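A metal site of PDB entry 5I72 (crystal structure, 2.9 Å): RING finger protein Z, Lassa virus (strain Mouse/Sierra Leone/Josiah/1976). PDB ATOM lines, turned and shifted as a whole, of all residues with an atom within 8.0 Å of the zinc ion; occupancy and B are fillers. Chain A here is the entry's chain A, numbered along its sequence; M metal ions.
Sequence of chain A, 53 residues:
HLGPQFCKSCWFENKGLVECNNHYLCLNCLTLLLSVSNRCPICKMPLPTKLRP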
ATOM      1  N   LYS A   8      24.949 -23.614  34.328  1.00  0.00           N
ATOM      2  CA  LYS A   8      23.690 -24.146  34.850  1.00  0.00           C
ATOM      3  C   LYS A   8      23.472 -25.607  34.454  1.00  0.00           C
ATOM      4  O   LYS A   8      22.532 -26.251  34.916  1.00  0.00           O
ATOM      5  CB  LYS A   8      22.509 -23.279  34.376  1.00  0.00           C
ATOM      6  CG  LYS A   8      21.275 -23.364  35.286  1.00  0.00           C
ATOM      7  CD  LYS A   8      20.125 -22.547  34.709  1.00  0.00           C
ATOM      8  CE  LYS A   8      18.915 -22.536  35.622  1.00  0.00           C
ATOM      9  NZ  LYS A   8      17.789 -21.768  35.003  1.00  0.00           N
ATOM     10  N   GLU A  19      27.533 -16.803  27.741  1.00  0.00           N
ATOM     11  CA  GLU A  19      26.233 -16.317  28.184  1.00  0.00           C
ATOM     12  C   GLU A  19      25.145 -16.992  27.356  1.00  0.00           C
ATOM     13  O   GLU A  19      24.985 -16.682  26.180  1.00  0.00           O
ATOM     14  CB  GLU A  19      26.146 -14.802  28.037  1.00  0.00           C
ATOM     15  CG  GLU A  19      26.059 -14.039  29.341  1.00  0.00           C
ATOM     16  CD  GLU A  19      25.554 -12.617  29.147  1.00  0.00           C
ATOM     17  OE1 GLU A  19      24.398 -12.451  28.714  1.00  0.00           O
ATOM     18  OE2 GLU A  19      26.319 -11.669  29.442  1.00  0.00           O
ATOM     19  N   CYS A  20      24.411 -17.908  27.973  1.00  0.00           N
ATOM     20  CA  CYS A  20      23.222 -18.436  27.322  1.00  0.00           C
ATOM     21  C   CYS A  20      22.100 -17.446  27.643  1.00  0.00           C
ATOM     22  O   CYS A  20      22.370 -16.394  28.231  1.00  0.00           O
ATOM     23  CB  CYS A  20      22.888 -19.852  27.801  1.00  0.00           C
ATOM     24  SG  CYS A  20      21.853 -20.823  26.660  1.00  0.00           S
ATOM     25  N   ASN A  21      20.871 -17.756  27.272  1.00  0.00           N
ATOM     26  CA  ASN A  21      19.844 -16.705  27.253  1.00  0.00           C
ATOM     27  C   ASN A  21      19.469 -16.159  28.633  1.00  0.00           C
ATOM     28  O   ASN A  21      19.381 -14.942  28.804  1.00  0.00           O
ATOM     29  CB  ASN A  21      18.613 -17.226  26.533  1.00  0.00           C
ATOM     30  CG  ASN A  21      18.915 -17.615  25.091  1.00  0.00           C
ATOM     31  OD1 ASN A  21      18.858 -16.777  24.195  1.00  0.00           O
ATOM     32  ND2 ASN A  21      19.248 -18.888  24.883  1.00  0.00           N
ATOM     33  N   ASN A  22      19.297 -17.025  29.632  1.00  0.00           N
ATOM     34  CA  ASN A  22      19.014 -16.543  30.988  1.00  0.00           C
ATOM     35  C   ASN A  22      19.840 -17.270  32.035  1.00  0.00           C
ATOM     36  O   ASN A  22      19.462 -17.333  33.210  1.00  0.00           O
ATOM     37  CB  ASN A  22      17.518 -16.653  31.311  1.00  0.00           C
ATOM     38  CG  ASN A  22      16.994 -18.079  31.253  1.00  0.00           C
ATOM     39  OD1 ASN A  22      17.737 -19.043  31.421  1.00  0.00           O
ATOM     40  ND2 ASN A  22      15.686 -18.205  31.021  1.00  0.00           N
ATOM     41  N   HIS A  23      20.974 -17.802  31.602  1.00  0.00           N
ATOM     42  CA  HIS A  23      21.868 -18.558  32.467  1.00  0.00           C
ATOM     43  C   HIS A  23      23.236 -18.657  31.817  1.00  0.00           C
ATOM     44  O   HIS A  23      23.460 -18.085  30.745  1.00  0.00           O
ATOM     45  CB  HIS A  23      21.312 -19.952  32.741  1.00  0.00           C
ATOM     46  CG  HIS A  23      21.247 -20.823  31.525  1.00  0.00           C
ATOM     47  ND1 HIS A  23      22.187 -21.791  31.249  1.00  0.00           N
ATOM     48  CD2 HIS A  23      20.356 -20.871  30.508  1.00  0.00           C
ATOM     49  CE1 HIS A  23      21.879 -22.396  30.119  1.00  0.00           C
ATOM     50  NE2 HIS A  23      20.772 -21.853  29.640  1.00  0.00           N
ATOM     51  N   TYR A  24      24.149 -19.369  32.453  1.00  0.00           N
ATOM     52  CA  TYR A  24      25.491 -19.548  31.901  1.00  0.00           C
ATOM     53  C   TYR A  24      25.740 -20.972  31.438  1.00  0.00           C
ATOM     54  O   TYR A  24      25.017 -21.893  31.784  1.00  0.00           O
ATOM     55  CB  TYR A  24      26.552 -19.146  32.939  1.00  0.00           C
ATOM     56  CG  TYR A  24      26.558 -17.682  33.278  1.00  0.00           C
ATOM     57  CD1 TYR A  24      27.097 -16.750  32.385  1.00  0.00           C
ATOM     58  CD2 TYR A  24      26.032 -17.214  34.478  1.00  0.00           C
ATOM     59  CE1 TYR A  24      27.116 -15.395  32.690  1.00  0.00           C
ATOM     60  CE2 TYR A  24      26.047 -15.868  34.792  1.00  0.00           C
ATOM     61  CZ  TYR A  24      26.589 -14.959  33.898  1.00  0.00           C
ATOM     62  OH  TYR A  24      26.601 -13.623  34.203  1.00  0.00           O
ATOM     63  N   LEU A  25      26.794 -21.133  30.632  1.00  0.00           N
ATOM     64  CA  LEU A  25      27.255 -22.444  30.200  1.00  0.00           C
ATOM     65  C   LEU A  25      28.770 -22.442  30.032  1.00  0.00           C
ATOM     66  O   LEU A  25      29.330 -21.538  29.408  1.00  0.00           O
ATOM     67  CB  LEU A  25      26.584 -22.859  28.884  1.00  0.00           C
ATOM     68  CG  LEU A  25      25.158 -23.400  28.938  1.00  0.00           C
ATOM     69  CD1 LEU A  25      24.657 -23.693  27.534  1.00  0.00           C
ATOM     70  CD2 LEU A  25      25.107 -24.655  29.789  1.00  0.00           C
ATOM     71  N   LEU A  30      28.532 -26.496  26.659  1.00  0.00           N
ATOM     72  CA  LEU A  30      27.980 -25.852  25.464  1.00  0.00           C
ATOM     73  C   LEU A  30      28.257 -26.686  24.214  1.00  0.00           C
ATOM     74  O   LEU A  30      27.392 -26.823  23.353  1.00  0.00           O
ATOM     75  CB  LEU A  30      28.563 -24.451  25.290  1.00  0.00           C
ATOM     76  CG  LEU A  30      28.190 -23.688  24.017  1.00  0.00           C
ATOM     77  CD1 LEU A  30      26.683 -23.690  23.803  1.00  0.00           C
ATOM     78  CD2 LEU A  30      28.724 -22.266  24.085  1.00  0.00           C
ATOM     79  N   LEU A  33      26.116 -29.859  24.185  1.00  0.00           N
ATOM     80  CA  LEU A  33      24.730 -29.488  23.904  1.00  0.00           C
ATOM     81  C   LEU A  33      24.550 -29.117  22.431  1.00  0.00           C
ATOM     82  O   LEU A  33      23.516 -29.426  21.837  1.00  0.00           O
ATOM     83  CB  LEU A  33      24.284 -28.326  24.790  1.00  0.00           C
ATOM     84  CG  LEU A  33      24.197 -28.558  26.304  1.00  0.00           C
ATOM     85  CD1 LEU A  33      23.823 -27.267  27.014  1.00  0.00           C
ATOM     86  CD2 LEU A  33      23.212 -29.672  26.647  1.00  0.00           C
ATOM     87  N   ARG A  39      18.847 -26.262  20.187  1.00  0.00           N
ATOM     88  CA  ARG A  39      17.988 -25.733  21.245  1.00  0.00           C
ATOM     89  C   ARG A  39      18.446 -26.211  22.629  1.00  0.00           C
ATOM     90  O   ARG A  39      18.688 -27.391  22.847  1.00  0.00           O
ATOM     91  CB  ARG A  39      16.537 -26.138  20.995  1.00  0.00           C
ATOM     92  CG  ARG A  39      15.591 -25.857  22.144  1.00  0.00           C
ATOM     93  CD  ARG A  39      14.154 -26.058  21.702  1.00  0.00           C
ATOM     94  NE  ARG A  39      13.582 -24.824  21.212  1.00  0.00           N
ATOM     95  CZ  ARG A  39      12.695 -24.748  20.230  1.00  0.00           C
ATOM     96  NH1 ARG A  39      12.272 -25.840  19.623  1.00  0.00           N
ATOM     97  NH2 ARG A  39      12.238 -23.560  19.846  1.00  0.00           N
ATOM     98  N   CYS A  40      18.539 -25.266  23.557  1.00  0.00           N
ATOM     99  CA  CYS A  40      19.027 -25.541  24.908  1.00  0.00           C
ATOM    100  C   CYS A  40      17.972 -26.274  25.738  1.00  0.00           C
ATOM    101  O   CYS A  40      16.818 -25.848  25.776  1.00  0.00           O
ATOM    102  CB  CYS A  40      19.453 -24.239  25.574  1.00  0.00           C
ATOM    103  SG  CYS A  40      20.042 -24.381  27.269  1.00  0.00           S
ATOM    104  N   PRO A  41      18.358 -27.361  26.408  1.00  0.00           N
ATOM    105  CA  PRO A  41      17.412 -28.142  27.194  1.00  0.00           C
ATOM    106  C   PRO A  41      17.120 -27.509  28.556  1.00  0.00           C
ATOM    107  O   PRO A  41      16.203 -27.936  29.256  1.00  0.00           O
ATOM    108  CB  PRO A  41      18.114 -29.486  27.367  1.00  0.00           C
ATOM    109  CG  PRO A  41      19.566 -29.116  27.386  1.00  0.00           C
ATOM    110  CD  PRO A  41      19.715 -27.937  26.460  1.00  0.00           C
ATOM    111  N   ILE A  42      17.897 -26.503  28.913  1.00  0.00           N
ATOM    112  CA  ILE A  42      17.757 -25.859  30.213  1.00  0.00           C
ATOM    113  C   ILE A  42      16.768 -24.703  30.178  1.00  0.00           C
ATOM    114  O   ILE A  42      15.963 -24.540  31.090  1.00  0.00           O
ATOM    115  CB  ILE A  42      19.113 -25.355  30.720  1.00  0.00           C
ATOM    116  CG1 ILE A  42      20.074 -26.517  30.945  1.00  0.00           C
ATOM    117  CG2 ILE A  42      18.942 -24.528  31.997  1.00  0.00           C
ATOM    118  CD1 ILE A  42      21.531 -26.108  31.006  1.00  0.00           C
ATOM    119  N   CYS A  43      16.826 -23.912  29.108  1.00  0.00           N
ATOM    120  CA  CYS A  43      16.001 -22.707  29.021  1.00  0.00           C
ATOM    121  C   CYS A  43      15.102 -22.703  27.787  1.00  0.00           C
ATOM    122  O   CYS A  43      14.367 -21.739  27.569  1.00  0.00           O
ATOM    123  CB  CYS A  43      16.894 -21.466  29.015  1.00  0.00           C
ATOM    124  SG  CYS A  43      17.883 -21.239  27.505  1.00  0.00           S
ATOM    125  N   LYS A  44      15.172 -23.765  26.991  1.00  0.00           N
ATOM    126  CA  LYS A  44      14.288 -23.992  25.837  1.00  0.00           C
ATOM    127  C   LYS A  44      14.529 -23.008  24.681  1.00  0.00           C
ATOM    128  O   LYS A  44      13.884 -23.112  23.638  1.00  0.00           O
ATOM    129  CB  LYS A  44      12.824 -23.937  26.306  1.00  0.00           C
ATOM    130  CG  LYS A  44      12.434 -25.103  27.207  1.00  0.00           C
ATOM    131  CD  LYS A  44      11.338 -24.753  28.202  1.00  0.00           C
ATOM    132  CE  LYS A  44      10.101 -24.199  27.526  1.00  0.00           C
ATOM    133  NZ  LYS A  44       9.005 -23.932  28.488  1.00  0.00           N
ATOM    134  N   MET A  45      15.481 -22.091  24.852  1.00  0.00           N
ATOM    135  CA  MET A  45      15.810 -21.111  23.814  1.00  0.00           C
ATOM    136  C   MET A  45      17.054 -21.511  23.015  1.00  0.00           C
ATOM    137  O   MET A  45      17.741 -22.473  23.394  1.00  0.00           O
ATOM    138  CB  MET A  45      15.975 -19.735  24.468  1.00  0.00           C
ATOM    139  CG  MET A  45      14.655 -19.091  24.838  1.00  0.00           C
ATOM    140  SD  MET A  45      14.829 -17.703  25.962  1.00  0.00           S
ATOM    141  CE  MET A  45      15.212 -18.553  27.492  1.00  0.00           C
ATOM    142  N   PRO A  46      17.356 -20.806  21.917  1.00  0.00           N
ATOM    143  CA  PRO A  46      18.495 -21.263  21.107  1.00  0.00           C
ATOM    144  C   PRO A  46      19.833 -21.153  21.808  1.00  0.00           C
ATOM    145  O   PRO A  46      20.072 -20.201  22.563  1.00  0.00           O
ATOM    146  CB  PRO A  46      18.445 -20.342  19.874  1.00  0.00           C
ATOM    147  CG  PRO A  46      17.658 -19.169  20.296  1.00  0.00           C
ATOM    148  CD  PRO A  46      16.632 -19.713  21.233  1.00  0.00           C
ATOM    149  N   LEU A  47      20.698 -22.126  21.563  1.00  0.00           N
ATOM    150  CA  LEU A  47      22.049 -22.143  22.108  1.00  0.00           C
ATOM    151  C   LEU A  47      22.922 -21.074  21.465  1.00  0.00           C
ATOM    152  O   LEU A  47      22.694 -20.687  20.314  1.00  0.00           O
ATOM    153  CB  LEU A  47      22.697 -23.519  21.931  1.00  0.00           C
ATOM    154  CG  LEU A  47      22.253 -24.605  22.906  1.00  0.00           C
ATOM    155  CD1 LEU A  47      22.505 -25.984  22.335  1.00  0.00           C
ATOM    156  CD2 LEU A  47      22.966 -24.428  24.231  1.00  0.00           C
ATOM    157  N   PRO A  48      23.913 -20.575  22.218  1.00  0.00           N
ATOM    158  CA  PRO A  48      24.893 -19.633  21.668  1.00  0.00           C
ATOM    159  C   PRO A  48      25.752 -20.310  20.594  1.00  0.00           C
ATOM    160  O   PRO A  48      26.285 -21.393  20.831  1.00  0.00           O
ATOM    161  CB  PRO A  48      25.729 -19.220  22.881  1.00  0.00           C
ATOM    162  CG  PRO A  48      24.902 -19.590  24.072  1.00  0.00           C
ATOM    163  CD  PRO A  48      24.135 -20.799  23.656  1.00  0.00           C
HETATM  164 ZN    ZN M   1      20.050 -21.975  27.727  1.00  0.00          ZN
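SG of Cys 40 sits close to N of Ile 42 (3.4 Å). The side-chain amide nitrogen of Asn 21 sits close to the side-chain sulfur of Cys 20 (3.7 Å). SG of Cys 43 lies close to N of Met 45, 3.7 Å away. The side-chain sulfur of Cys 43 sits close to the side-chain amide nitrogen of Asn 21 (3.8 Å). The backbone carbonyl oxygen (O) of Met 45 lies within hydrogen-bond range of the backbone NH (N) of Cys 40.
The nearest printed residue that does not touch the zinc ion is Asn 21 (4.3 Å).
The zinc ion is bound by NE2 of His 23 (2.0 Å), SG of Cys 43 (2.3 Å), SG of Cys 20 (2.4 Å) and SG of Cys 40 (2.4 Å). The zinc ion has four donor atoms within binding distance.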
